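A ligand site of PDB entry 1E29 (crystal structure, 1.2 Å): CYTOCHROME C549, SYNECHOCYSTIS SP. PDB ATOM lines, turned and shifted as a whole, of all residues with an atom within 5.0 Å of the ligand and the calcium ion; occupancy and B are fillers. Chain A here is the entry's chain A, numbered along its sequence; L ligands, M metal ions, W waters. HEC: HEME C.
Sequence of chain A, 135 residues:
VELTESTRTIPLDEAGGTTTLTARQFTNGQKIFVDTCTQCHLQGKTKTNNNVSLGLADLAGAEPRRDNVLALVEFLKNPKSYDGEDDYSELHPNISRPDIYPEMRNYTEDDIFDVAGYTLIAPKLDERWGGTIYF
The calcium ion is bound by water W3. The calcium ion is bound by water W5 (2.4 Å). Water W6 is bound to the calcium ion (2.4 Å). Water W4 binds the calcium ion (2.4 Å). The calcium ion is bound by water W7, 2.4 Å away. OD1 of Asn 49 is bound to the calcium ion (2.5 Å). The calcium ion is bound by the side-chain amide oxygen (OD1) of Asn 50 (2.5 Å).
Water W1 lies within hydrogen-bond range of O1D of the ligand, N of Tyr 82 and OH of Tyr 88. Water W2 lies within hydrogen-bond range of the backbone carbonyl oxygen (O) of Lys 80, an oxygen (O1D) of the ligand, the guanidinium group (NH1) of Arg 66 and the backbone NH (N) of Tyr 82.
Thr 36 touches the ligand. Gln 39 touches the ligand. OG1 of Thr 48 touches CMD of the ligand, 3.4 Å away. C of Val 52 touches O2A of the ligand, 3.5 Å away. CD2 of Leu 54 touches C3A of the ligand, at 3.4 Å. C of Asp 58 touches O2A of the ligand, 3.5 Å away. Leu 59 touches the ligand. Ala 62 touches the ligand (CB to O1A, 3.7 Å). Leu 72 touches the ligand (CD2 to CMA, 3.4 Å). CE2 of Phe 75 touches C3A of the ligand (3.4 Å). CD2 of Leu 76 touches C2B of the ligand, at 3.9 Å. Tyr 82 touches the ligand (CE1 to O1A, 3.4 Å). Tyr 88 touches the ligand (CE2 to O1D, 3.9 Å). CG of Pro 93 touches CMC of the ligand, at 3.8 Å. Hydrophobic or aromatic side chains within 4 Å of the ligand: His 41, Val 52, Leu 54, Leu 59, Ala 62, Leu 72, Phe 75, Leu 76, Tyr 82, Tyr 88, His 92 and Pro 93. 21 residues have an atom within 4 Å of the ligand: Thr 36, Cys 37, Gln 39, Cys 40, His 41, Thr 48, Asn 49, Val 52, Ser 53, Leu 54, Asp 58, Leu 59, Ala 62, Arg 66, Leu 72, Phe 75, Leu 76, Tyr 82, Tyr 88, His 92 and Pro 93.
The side-chain sulfur (SG) of Cys 37 is bonded to a carbon (CAB) of the ligand, at 1.8 Å. The side-chain sulfur (SG) of Cys 40 is bonded to a carbon (CAC) of the ligand (1.8 Å). FE of the ligand is bound by NE2 of His 41 (2.0 Å). NE2 of His 92 binds FE of the ligand, 2.0 Å away. ND2 of Asn 49 lies within hydrogen-bond range of O2D of the ligand (2.8 Å). O of Ser 53 lies close to O2A of the ligand (2.5 Å). The guanidinium group of Arg 66 is in salt-bridge range of an oxygen (O1A) of the ligand (2.9 Å).
A ring nitrogen (ND1) of His 41 is in hydrogen-bond range of the side-chain hydroxyl of Thr 46, at 3.1 Å. The side-chain hydroxyl (OG) of Ser 53 is in hydrogen-bond range of the side-chain carboxylate (OD2) of Asp 58, at 2.7 Å. The backbone NH (N) of Arg 66 is in hydrogen-bond range of the backbone carbonyl oxygen (O) of Leu 59 (2.8 Å). The guanidinium group (NH2) of Arg 66 is in hydrogen-bond range of the backbone carbonyl oxygen (O) of Ser 81 (3.0 Å). The guanidinium group of Arg 66 lies within hydrogen-bond range of the backbone carbonyl oxygen of Lys 80 (3.3 Å). OH of Tyr 82 is in hydrogen-bond range of O of Asp 58 (2.6 Å). The backbone carbonyl oxygen (O) of Thr 36 sits at hydrogen-bond distance from the side-chain amide nitrogen (NE2) of Gln 39, at 3.2 Å. The side-chain hydroxyl (OG1) of Thr 46 sits at hydrogen-bond distance from the backbone carbonyl oxygen (O) of Val 52 (2.9 Å).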
ATOM      1  N   PHE A  33      -2.040  19.615  26.963  1.00  0.00           N
ATOM      2  CA  PHE A  33      -2.169  18.199  26.636  1.00  0.00           C
ATOM      3  C   PHE A  33      -1.356  17.352  27.656  1.00  0.00           C
ATOM      4  O   PHE A  33      -1.832  16.347  28.181  1.00  0.00           O
ATOM      5  CB  PHE A  33      -1.826  17.950  25.169  1.00  0.00           C
ATOM      6  CG  PHE A  33      -2.210  16.574  24.715  1.00  0.00           C
ATOM      7  CD1 PHE A  33      -1.376  15.474  24.975  1.00  0.00           C
ATOM      8  CD2 PHE A  33      -3.425  16.381  24.087  1.00  0.00           C
ATOM      9  CE1 PHE A  33      -1.816  14.230  24.576  1.00  0.00           C
ATOM     10  CE2 PHE A  33      -3.830  15.114  23.718  1.00  0.00           C
ATOM     11  CZ  PHE A  33      -3.047  14.029  23.993  1.00  0.00           C
ATOM     12  N   THR A  36      -3.004  17.507  31.255  1.00  0.00           N
ATOM     13  CA  THR A  36      -4.382  17.120  31.518  1.00  0.00           C
ATOM     14  C   THR A  36      -4.846  15.967  30.666  1.00  0.00           C
ATOM     15  O   THR A  36      -5.821  15.300  31.028  1.00  0.00           O
ATOM     16  CB  THR A  36      -5.259  18.387  31.310  1.00  0.00           C
ATOM     17  OG1 THR A  36      -4.830  19.338  32.292  1.00  0.00           O
ATOM     18  CG2 THR A  36      -6.716  18.116  31.530  1.00  0.00           C
ATOM     19  N   CYS A  37      -4.283  15.683  29.494  1.00  0.00           N
ATOM     20  CA  CYS A  37      -4.774  14.707  28.548  1.00  0.00           C
ATOM     21  C   CYS A  37      -3.940  13.417  28.548  1.00  0.00           C
ATOM     22  O   CYS A  37      -4.465  12.358  28.193  1.00  0.00           O
ATOM     23  CB  CYS A  37      -4.864  15.239  27.120  1.00  0.00           C
ATOM     24  SG  CYS A  37      -5.638  16.856  27.002  1.00  0.00           S
ATOM     25  N   GLN A  39      -2.857  11.517  30.842  1.00  0.00           N
ATOM     26  CA  GLN A  39      -3.251  10.441  31.748  1.00  0.00           C
ATOM     27  C   GLN A  39      -4.081   9.373  31.052  1.00  0.00           C
ATOM     28  O   GLN A  39      -4.049   8.221  31.495  1.00  0.00           O
ATOM     29  CB  GLN A  39      -3.989  11.013  32.923  1.00  0.00           C
ATOM     30  CG  GLN A  39      -4.678  12.309  32.865  1.00  0.00           C
ATOM     31  CD  GLN A  39      -5.560  12.708  34.023  1.00  0.00           C
ATOM     32  OE1 GLN A  39      -5.952  11.917  34.885  1.00  0.00           O
ATOM     33  NE2 GLN A  39      -5.875  14.026  33.947  1.00  0.00           N
ATOM     34  N   CYS A  40      -4.793   9.708  30.004  1.00  0.00           N
ATOM     35  CA  CYS A  40      -5.554   8.717  29.233  1.00  0.00           C
ATOM     36  C   CYS A  40      -5.169   8.638  27.765  1.00  0.00           C
ATOM     37  O   CYS A  40      -5.552   7.655  27.096  1.00  0.00           O
ATOM     38  CB  CYS A  40      -7.031   9.008  29.385  1.00  0.00           C
ATOM     39  SG  CYS A  40      -7.553   8.940  31.126  1.00  0.00           S
ATOM     40  N   HIS A  41      -4.497   9.659  27.250  1.00  0.00           N
ATOM     41  CA  HIS A  41      -4.179   9.711  25.820  1.00  0.00           C
ATOM     42  C   HIS A  41      -2.685   9.963  25.584  1.00  0.00           C
ATOM     43  O   HIS A  41      -2.291  10.713  24.677  1.00  0.00           O
ATOM     44  CB  HIS A  41      -4.958  10.821  25.100  1.00  0.00           C
ATOM     45  CG  HIS A  41      -6.427  10.675  25.148  1.00  0.00           C
ATOM     46  ND1 HIS A  41      -7.161   9.637  24.614  1.00  0.00           N
ATOM     47  CD2 HIS A  41      -7.345  11.542  25.687  1.00  0.00           C
ATOM     48  CE1 HIS A  41      -8.410   9.918  24.853  1.00  0.00           C
ATOM     49  NE2 HIS A  41      -8.627  11.057  25.499  1.00  0.00           N
ATOM     50  N   THR A  46      -5.856   5.690  22.672  1.00  0.00           N
ATOM     51  CA  THR A  46      -6.922   5.356  23.583  1.00  0.00           C
ATOM     52  C   THR A  46      -6.852   3.848  23.774  1.00  0.00           C
ATOM     53  O   THR A  46      -6.528   3.064  22.856  1.00  0.00           O
ATOM     54  CB  THR A  46      -8.278   5.801  22.989  1.00  0.00           C
ATOM     55  OG1 THR A  46      -8.345   7.242  22.954  1.00  0.00           O
ATOM     56  CG2 THR A  46      -9.443   5.228  23.777  1.00  0.00           C
ATOM     57  N   THR A  48      -9.266   2.110  26.100  1.00  0.00           N
ATOM     58  CA  THR A  48     -10.464   1.495  26.629  1.00  0.00           C
ATOM     59  C   THR A  48     -11.592   1.500  25.591  1.00  0.00           C
ATOM     60  O   THR A  48     -12.737   1.120  25.897  1.00  0.00           O
ATOM     61  CB  THR A  48     -10.912   2.122  27.972  1.00  0.00           C
ATOM     62  OG1 THR A  48     -11.007   3.553  27.751  1.00  0.00           O
ATOM     63  CG2 THR A  48      -9.929   1.830  29.096  1.00  0.00           C
ATOM     64  N   ASN A  49     -11.313   1.835  24.347  1.00  0.00           N
ATOM     65  CA  ASN A  49     -12.286   1.649  23.258  1.00  0.00           C
ATOM     66  C   ASN A  49     -11.431   1.448  22.005  1.00  0.00           C
ATOM     67  O   ASN A  49     -10.280   1.858  21.973  1.00  0.00           O
ATOM     68  CB  ASN A  49     -13.304   2.763  23.102  1.00  0.00           C
ATOM     69  CG  ASN A  49     -14.591   2.398  22.385  1.00  0.00           C
ATOM     70  OD1 ASN A  49     -14.702   1.319  21.783  1.00  0.00           O
ATOM     71  ND2 ASN A  49     -15.584   3.281  22.490  1.00  0.00           N
ATOM     72  N   ASN A  50     -11.982   0.812  20.997  1.00  0.00           N
ATOM     73  CA  ASN A  50     -11.313   0.542  19.734  1.00  0.00           C
ATOM     74  C   ASN A  50     -11.678   1.639  18.732  1.00  0.00           C
ATOM     75  O   ASN A  50     -12.845   2.012  18.577  1.00  0.00           O
ATOM     76  CB  ASN A  50     -11.684  -0.810  19.196  1.00  0.00           C
ATOM     77  CG  ASN A  50     -13.169  -1.076  19.079  1.00  0.00           C
ATOM     78  OD1 ASN A  50     -13.968  -0.668  19.912  1.00  0.00           O
ATOM     79  ND2 ASN A  50     -13.587  -1.844  18.069  1.00  0.00           N
ATOM     80  N   ASN A  51     -10.661   2.091  18.051  1.00  0.00           N
ATOM     81  CA  ASN A  51     -10.720   3.121  17.027  1.00  0.00           C
ATOM     82  C   ASN A  51     -11.355   4.421  17.492  1.00  0.00           C
ATOM     83  O   ASN A  51     -12.091   5.096  16.781  1.00  0.00           O
ATOM     84  CB  ASN A  51     -11.477   2.500  15.827  1.00  0.00           C
ATOM     85  CG  ASN A  51     -10.894   1.123  15.480  1.00  0.00           C
ATOM     86  OD1 ASN A  51      -9.685   1.022  15.296  1.00  0.00           O
ATOM     87  ND2 ASN A  51     -11.731   0.081  15.426  1.00  0.00           N
ATOM     88  N   VAL A  52     -11.077   4.804  18.748  1.00  0.00           N
ATOM     89  CA  VAL A  52     -11.543   6.080  19.255  1.00  0.00           C
ATOM     90  C   VAL A  52     -10.361   6.797  19.866  1.00  0.00           C
ATOM     91  O   VAL A  52     -10.367   7.389  20.934  1.00  0.00           O
ATOM     92  CB  VAL A  52     -12.651   5.916  20.302  1.00  0.00           C
ATOM     93  CG1 VAL A  52     -13.194   7.275  20.686  1.00  0.00           C
ATOM     94  CG2 VAL A  52     -13.797   5.079  19.727  1.00  0.00           C
ATOM     95  N   SER A  53      -9.262   6.777  19.132  1.00  0.00           N
ATOM     96  CA  SER A  53      -8.055   7.474  19.495  1.00  0.00           C
ATOM     97  C   SER A  53      -8.086   8.911  19.008  1.00  0.00           C
ATOM     98  O   SER A  53      -9.046   9.418  18.422  1.00  0.00           O
ATOM     99  CB  SER A  53      -6.810   6.734  19.003  1.00  0.00           C
ATOM    100  OG  SER A  53      -6.497   6.990  17.658  1.00  0.00           O
ATOM    101  N   LEU A  54      -6.957   9.597  19.267  1.00  0.00           N
ATOM    102  CA  LEU A  54      -6.807  10.968  18.741  1.00  0.00           C
ATOM    103  C   LEU A  54      -6.097  11.009  17.385  1.00  0.00           C
ATOM    104  O   LEU A  54      -5.702  12.051  16.899  1.00  0.00           O
ATOM    105  CB  LEU A  54      -6.093  11.832  19.773  1.00  0.00           C
ATOM    106  CG  LEU A  54      -6.584  11.804  21.221  1.00  0.00           C
ATOM    107  CD1 LEU A  54      -5.985  12.929  22.072  1.00  0.00           C
ATOM    108  CD2 LEU A  54      -8.087  11.897  21.296  1.00  0.00           C
ATOM    109  N   ASP A  58      -9.406   8.100  13.179  1.00  0.00           N
ATOM    110  CA  ASP A  58     -10.377   7.831  14.230  1.00  0.00           C
ATOM    111  C   ASP A  58     -11.253   9.060  14.459  1.00  0.00           C
ATOM    112  O   ASP A  58     -12.477   9.032  14.512  1.00  0.00           O
ATOM    113  CB  ASP A  58      -9.707   7.423  15.558  1.00  0.00           C
ATOM    114  CG  ASP A  58      -9.178   5.997  15.525  1.00  0.00           C
ATOM    115  OD1 ASP A  58      -9.449   5.250  14.545  1.00  0.00           O
ATOM    116  OD2 ASP A  58      -8.496   5.611  16.502  1.00  0.00           O
ATOM    117  N   LEU A  59     -10.591  10.240  14.558  1.00  0.00           N
ATOM    118  CA  LEU A  59     -11.353  11.471  14.740  1.00  0.00           C
ATOM    119  C   LEU A  59     -12.379  11.696  13.594  1.00  0.00           C
ATOM    120  O   LEU A  59     -13.517  12.137  13.842  1.00  0.00           O
ATOM    121  CB  LEU A  59     -10.431  12.649  14.867  1.00  0.00           C
ATOM    122  CG  LEU A  59      -9.534  12.710  16.111  1.00  0.00           C
ATOM    123  CD1 LEU A  59      -8.547  13.870  15.944  1.00  0.00           C
ATOM    124  CD2 LEU A  59     -10.336  12.883  17.370  1.00  0.00           C
ATOM    125  N   ALA A  62     -15.779   9.971  13.886  1.00  0.00           N
ATOM    126  CA  ALA A  62     -16.720  10.354  14.915  1.00  0.00           C
ATOM    127  C   ALA A  62     -17.915  11.069  14.291  1.00  0.00           C
ATOM    128  O   ALA A  62     -17.854  11.485  13.120  1.00  0.00           O
ATOM    129  CB  ALA A  62     -16.044  11.184  15.999  1.00  0.00           C
ATOM    130  N   ARG A  66     -14.450  14.776  14.034  1.00  0.00           N
ATOM    131  CA  ARG A  66     -13.687  15.517  15.037  1.00  0.00           C
ATOM    132  C   ARG A  66     -12.288  15.913  14.568  1.00  0.00           C
ATOM    133  O   ARG A  66     -11.433  16.334  15.340  1.00  0.00           O
ATOM    134  CB  ARG A  66     -13.622  14.678  16.344  1.00  0.00           C
ATOM    135  CG  ARG A  66     -14.998  14.575  17.031  1.00  0.00           C
ATOM    136  CD  ARG A  66     -14.997  13.558  18.177  1.00  0.00           C
ATOM    137  NE  ARG A  66     -16.326  13.388  18.729  1.00  0.00           N
ATOM    138  CZ  ARG A  66     -16.711  12.389  19.493  1.00  0.00           C
ATOM    139  NH1 ARG A  66     -15.844  11.387  19.776  1.00  0.00           N
ATOM    140  NH2 ARG A  66     -17.956  12.372  19.951  1.00  0.00           N
ATOM    141  N   LEU A  72     -13.524  19.731  17.791  1.00  0.00           N
ATOM    142  CA  LEU A  72     -12.783  19.359  18.996  1.00  0.00           C
ATOM    143  C   LEU A  72     -13.110  20.287  20.121  1.00  0.00           C
ATOM    144  O   LEU A  72     -13.268  19.854  21.264  1.00  0.00           O
ATOM    145  CB  LEU A  72     -11.293  19.292  18.702  1.00  0.00           C
ATOM    146  CG  LEU A  72     -10.816  18.067  17.940  1.00  0.00           C
ATOM    147  CD1 LEU A  72      -9.353  18.236  17.583  1.00  0.00           C
ATOM    148  CD2 LEU A  72     -11.017  16.829  18.759  1.00  0.00           C
ATOM    149  N   PHE A  75     -16.363  19.208  21.399  1.00  0.00           N
ATOM    150  CA  PHE A  75     -16.253  17.969  22.165  1.00  0.00           C
ATOM    151  C   PHE A  75     -15.775  18.269  23.590  1.00  0.00           C
ATOM    152  O   PHE A  75     -16.213  17.660  24.567  1.00  0.00           O
ATOM    153  CB  PHE A  75     -15.327  16.995  21.475  1.00  0.00           C
ATOM    154  CG  PHE A  75     -15.146  15.683  22.206  1.00  0.00           C
ATOM    155  CD1 PHE A  75     -16.053  14.649  22.059  1.00  0.00           C
ATOM    156  CD2 PHE A  75     -14.080  15.510  23.103  1.00  0.00           C
ATOM    157  CE1 PHE A  75     -15.847  13.441  22.702  1.00  0.00           C
ATOM    158  CE2 PHE A  75     -13.928  14.300  23.775  1.00  0.00           C
ATOM    159  CZ  PHE A  75     -14.820  13.281  23.578  1.00  0.00           C
ATOM    160  N   LEU A  76     -14.809  19.187  23.739  1.00  0.00           N
ATOM    161  CA  LEU A  76     -14.227  19.495  25.036  1.00  0.00           C
ATOM    162  C   LEU A  76     -15.071  20.383  25.890  1.00  0.00           C
ATOM    163  O   LEU A  76     -14.830  20.568  27.104  1.00  0.00           O
ATOM    164  CB  LEU A  76     -12.793  20.077  24.873  1.00  0.00           C
ATOM    165  CG  LEU A  76     -11.805  19.057  24.350  1.00  0.00           C
ATOM    166  CD1 LEU A  76     -10.489  19.778  23.989  1.00  0.00           C
ATOM    167  CD2 LEU A  76     -11.551  17.958  25.370  1.00  0.00           C
ATOM    168  N   LYS A  80     -19.303  13.603  23.938  1.00  0.00           N
ATOM    169  CA  LYS A  80     -20.290  12.613  23.582  1.00  0.00           C
ATOM    170  C   LYS A  80     -19.615  11.267  23.272  1.00  0.00           C
ATOM    171  O   LYS A  80     -18.413  11.268  23.041  1.00  0.00           O
ATOM    172  CB  LYS A  80     -21.050  12.969  22.302  1.00  0.00           C
ATOM    173  CG  LYS A  80     -21.696  14.342  22.316  1.00  0.00           C
ATOM    174  CD  LYS A  80     -22.874  14.377  23.244  1.00  0.00           C
ATOM    175  CE  LYS A  80     -23.878  15.425  22.794  1.00  0.00           C
ATOM    176  NZ  LYS A  80     -23.496  16.787  23.245  1.00  0.00           N
ATOM    177  N   SER A  81     -20.404  10.203  23.267  1.00  0.00           N
ATOM    178  CA  SER A  81     -19.871   8.934  22.731  1.00  0.00           C
ATOM    179  C   SER A  81     -19.533   9.142  21.255  1.00  0.00           C
ATOM    180  O   SER A  81     -19.859  10.149  20.594  1.00  0.00           O
ATOM    181  CB  SER A  81     -20.940   7.871  22.969  1.00  0.00           C
ATOM    182  OG  SER A  81     -22.031   8.213  22.166  1.00  0.00           O
ATOM    183  N   TYR A  82     -18.855   8.143  20.702  1.00  0.00           N
ATOM    184  CA  TYR A  82     -18.292   8.316  19.360  1.00  0.00           C
ATOM    185  C   TYR A  82     -19.322   8.466  18.280  1.00  0.00           C
ATOM    186  O   TYR A  82     -19.105   9.162  17.289  1.00  0.00           O
ATOM    187  CB  TYR A  82     -17.491   7.051  19.099  1.00  0.00           C
ATOM    188  CG  TYR A  82     -16.639   7.043  17.851  1.00  0.00           C
ATOM    189  CD1 TYR A  82     -15.567   7.922  17.759  1.00  0.00           C
ATOM    190  CD2 TYR A  82     -16.861   6.235  16.773  1.00  0.00           C
ATOM    191  CE1 TYR A  82     -14.776   7.932  16.646  1.00  0.00           C
ATOM    192  CE2 TYR A  82     -16.105   6.204  15.614  1.00  0.00           C
ATOM    193  CZ  TYR A  82     -15.036   7.102  15.568  1.00  0.00           C
ATOM    194  OH  TYR A  82     -14.253   7.094  14.444  1.00  0.00           O
ATOM    195  N   TYR A  88     -21.533  12.547  27.496  1.00  0.00           N
ATOM    196  CA  TYR A  88     -20.381  12.196  28.315  1.00  0.00           C
ATOM    197  C   TYR A  88     -19.942  13.350  29.185  1.00  0.00           C
ATOM    198  O   TYR A  88     -18.791  13.392  29.635  1.00  0.00           O
ATOM    199  CB  TYR A  88     -19.251  11.706  27.408  1.00  0.00           C
ATOM    200  CG  TYR A  88     -19.332  10.268  26.945  1.00  0.00           C
ATOM    201  CD1 TYR A  88     -20.436   9.419  27.128  1.00  0.00           C
ATOM    202  CD2 TYR A  88     -18.223   9.740  26.279  1.00  0.00           C
ATOM    203  CE1 TYR A  88     -20.462   8.110  26.666  1.00  0.00           C
ATOM    204  CE2 TYR A  88     -18.263   8.441  25.849  1.00  0.00           C
ATOM    205  CZ  TYR A  88     -19.363   7.627  26.034  1.00  0.00           C
ATOM    206  OH  TYR A  88     -19.359   6.326  25.544  1.00  0.00           O
ATOM    207  N   HIS A  92     -16.355  12.196  30.584  1.00  0.00           N
ATOM    208  CA  HIS A  92     -15.137  12.656  29.971  1.00  0.00           C
ATOM    209  C   HIS A  92     -14.811  14.070  30.446  1.00  0.00           C
ATOM    210  O   HIS A  92     -15.701  14.917  30.422  1.00  0.00           O
ATOM    211  CB  HIS A  92     -15.262  12.653  28.420  1.00  0.00           C
ATOM    212  CG  HIS A  92     -13.964  12.928  27.738  1.00  0.00           C
ATOM    213  ND1 HIS A  92     -13.382  14.167  27.661  1.00  0.00           N
ATOM    214  CD2 HIS A  92     -13.100  12.070  27.177  1.00  0.00           C
ATOM    215  CE1 HIS A  92     -12.196  14.010  27.048  1.00  0.00           C
ATOM    216  NE2 HIS A  92     -11.993  12.765  26.738  1.00  0.00           N
ATOM    217  N   PRO A  93     -13.558  14.376  30.786  1.00  0.00           N
ATOM    218  CA  PRO A  93     -13.229  15.752  31.199  1.00  0.00           C
ATOM    219  C   PRO A  93     -13.659  16.796  30.196  1.00  0.00           C
ATOM    220  O   PRO A  93     -13.587  16.633  28.982  1.00  0.00           O
ATOM    221  CB  PRO A  93     -11.681  15.718  31.364  1.00  0.00           C
ATOM    222  CG  PRO A  93     -11.423  14.283  31.703  1.00  0.00           C
ATOM    223  CD  PRO A  93     -12.363  13.499  30.850  1.00  0.00           C
ATOM    224  N   MET A 104      -9.808  21.256  34.792  1.00  0.00           N
ATOM    225  CA  MET A 104     -10.246  21.951  33.610  1.00  0.00           C
ATOM    226  C   MET A 104     -10.732  23.349  33.969  1.00  0.00           C
ATOM    227  O   MET A 104     -11.022  24.098  33.050  1.00  0.00           O
ATOM    228  CB  MET A 104     -11.356  21.173  32.913  1.00  0.00           C
ATOM    229  CG  MET A 104     -11.119  19.740  32.457  1.00  0.00           C
ATOM    230  SD  MET A 104     -10.029  19.608  31.049  1.00  0.00           S
ATOM    231  CE  MET A 104     -10.951  20.106  29.630  1.00  0.00           C
ATOM    232  N   VAL A 115      -5.557  23.554  22.586  1.00  0.00           N
ATOM    233  CA  VAL A 115      -5.310  22.095  22.693  1.00  0.00           C
ATOM    234  C   VAL A 115      -5.942  21.405  21.513  1.00  0.00           C
ATOM    235  O   VAL A 115      -5.392  20.393  21.039  1.00  0.00           O
ATOM    236  CB  VAL A 115      -5.662  21.663  24.127  1.00  0.00           C
ATOM    237  CG1 VAL A 115      -7.104  21.687  24.370  1.00  0.00           C
ATOM    238  CG2 VAL A 115      -5.121  20.234  24.344  1.00  0.00           C
ATOM    239  N   THR A 119      -3.860  18.996  19.007  1.00  0.00           N
ATOM    240  CA  THR A 119      -4.253  17.616  18.760  1.00  0.00           C
ATOM    241  C   THR A 119      -4.199  17.277  17.278  1.00  0.00           C
ATOM    242  O   THR A 119      -3.862  16.184  16.892  1.00  0.00           O
ATOM    243  CB  THR A 119      -5.657  17.390  19.365  1.00  0.00           C
ATOM    244  OG1 THR A 119      -5.585  17.539  20.789  1.00  0.00           O
ATOM    245  CG2 THR A 119      -6.186  16.011  19.052  1.00  0.00           C
HETATM  246 FE   HEC L   1     -10.284  11.943  26.085  1.00  0.00          FE
HETATM  247  CHA HEC L   1     -12.026  10.170  23.837  1.00  0.00           C
HETATM  248  CHB HEC L   1      -9.765  14.350  23.788  1.00  0.00           C
HETATM  249  CHC HEC L   1      -8.600  13.838  28.368  1.00  0.00           C
HETATM  250  CHD HEC L   1     -10.545   9.445  28.313  1.00  0.00           C
HETATM  251  NA  HEC L   1     -10.871  12.246  24.222  1.00  0.00           N
HETATM  252  C1A HEC L   1     -11.584  11.397  23.407  1.00  0.00           C
HETATM  253  C2A HEC L   1     -11.789  11.974  22.109  1.00  0.00           C
HETATM  254  C3A HEC L   1     -11.175  13.188  22.108  1.00  0.00           C
HETATM  255  C4A HEC L   1     -10.552  13.326  23.400  1.00  0.00           C
HETATM  256  CMA HEC L   1     -11.111  14.227  20.998  1.00  0.00           C
HETATM  257  CAA HEC L   1     -12.538  11.340  20.953  1.00  0.00           C
HETATM  258  CBA HEC L   1     -11.641  10.566  20.014  1.00  0.00           C
HETATM  259  CGA HEC L   1     -12.244  10.123  18.679  1.00  0.00           C
HETATM  260  O1A HEC L   1     -13.427  10.431  18.438  1.00  0.00           O
HETATM  261  O2A HEC L   1     -11.525   9.396  17.917  1.00  0.00           O
HETATM  262  NB  HEC L   1      -9.377  13.730  26.068  1.00  0.00           N
HETATM  263  C1B HEC L   1      -9.174  14.562  24.985  1.00  0.00           C
HETATM  264  C2B HEC L   1      -8.354  15.702  25.329  1.00  0.00           C
HETATM  265  C3B HEC L   1      -8.133  15.591  26.680  1.00  0.00           C
HETATM  266  C4B HEC L   1      -8.732  14.366  27.117  1.00  0.00           C
HETATM  267  CMB HEC L   1      -7.841  16.748  24.351  1.00  0.00           C
HETATM  268  CAB HEC L   1      -7.337  16.570  27.532  1.00  0.00           C
HETATM  269  CBB HEC L   1      -8.034  17.911  27.663  1.00  0.00           C
HETATM  270  NC  HEC L   1      -9.734  11.722  27.980  1.00  0.00           N
HETATM  271  C1C HEC L   1      -9.026  12.584  28.804  1.00  0.00           C
HETATM  272  C2C HEC L   1      -8.800  12.007  30.114  1.00  0.00           C
HETATM  273  C3C HEC L   1      -9.337  10.765  30.102  1.00  0.00           C
HETATM  274  C4C HEC L   1      -9.915  10.590  28.771  1.00  0.00           C
HETATM  275  CMC HEC L   1      -7.986  12.736  31.185  1.00  0.00           C
HETATM  276  CAC HEC L   1      -9.234   9.627  31.106  1.00  0.00           C
HETATM  277  CBC HEC L   1      -9.574  10.093  32.499  1.00  0.00           C
HETATM  278  ND  HEC L   1     -11.130  10.151  26.101  1.00  0.00           N
HETATM  279  C1D HEC L   1     -11.084   9.192  27.088  1.00  0.00           C
HETATM  280  C2D HEC L   1     -11.792   8.018  26.694  1.00  0.00           C
HETATM  281  C3D HEC L   1     -12.263   8.233  25.440  1.00  0.00           C
HETATM  282  C4D HEC L   1     -11.806   9.564  25.058  1.00  0.00           C
HETATM  283  CMD HEC L   1     -11.931   6.767  27.547  1.00  0.00           C
HETATM  284  CAD HEC L   1     -13.124   7.371  24.562  1.00  0.00           C
HETATM  285  CBD HEC L   1     -14.606   7.690  24.573  1.00  0.00           C
HETATM  286  CGD HEC L   1     -15.417   6.673  23.801  1.00  0.00           C
HETATM  287  O1D HEC L   1     -16.160   7.093  22.891  1.00  0.00           O
HETATM  288  O2D HEC L   1     -15.333   5.473  24.148  1.00  0.00           O
HETATM  289 CA    CA M   1     -16.317  -0.110  20.591  1.00  0.00          CA
HETATM  290  O   HOH W   1     -18.352   5.894  22.521  1.00  0.00           O
HETATM  291  O   HOH W   2     -16.399   9.708  22.010  1.00  0.00           O
HETATM  292  O   HOH W   3     -18.542  -0.777  20.353  1.00  0.00           O
HETATM  293  O   HOH W   4     -15.735   1.626  19.024  1.00  0.00           O
HETATM  294  O   HOH W   5     -15.832  -2.397  20.970  1.00  0.00           O
HETATM  295  O   HOH W   6     -17.585   1.911  20.463  1.00  0.00           O
HETATM  296  O   HOH W   7     -16.722  -1.045  18.372  1.00  0.00           O
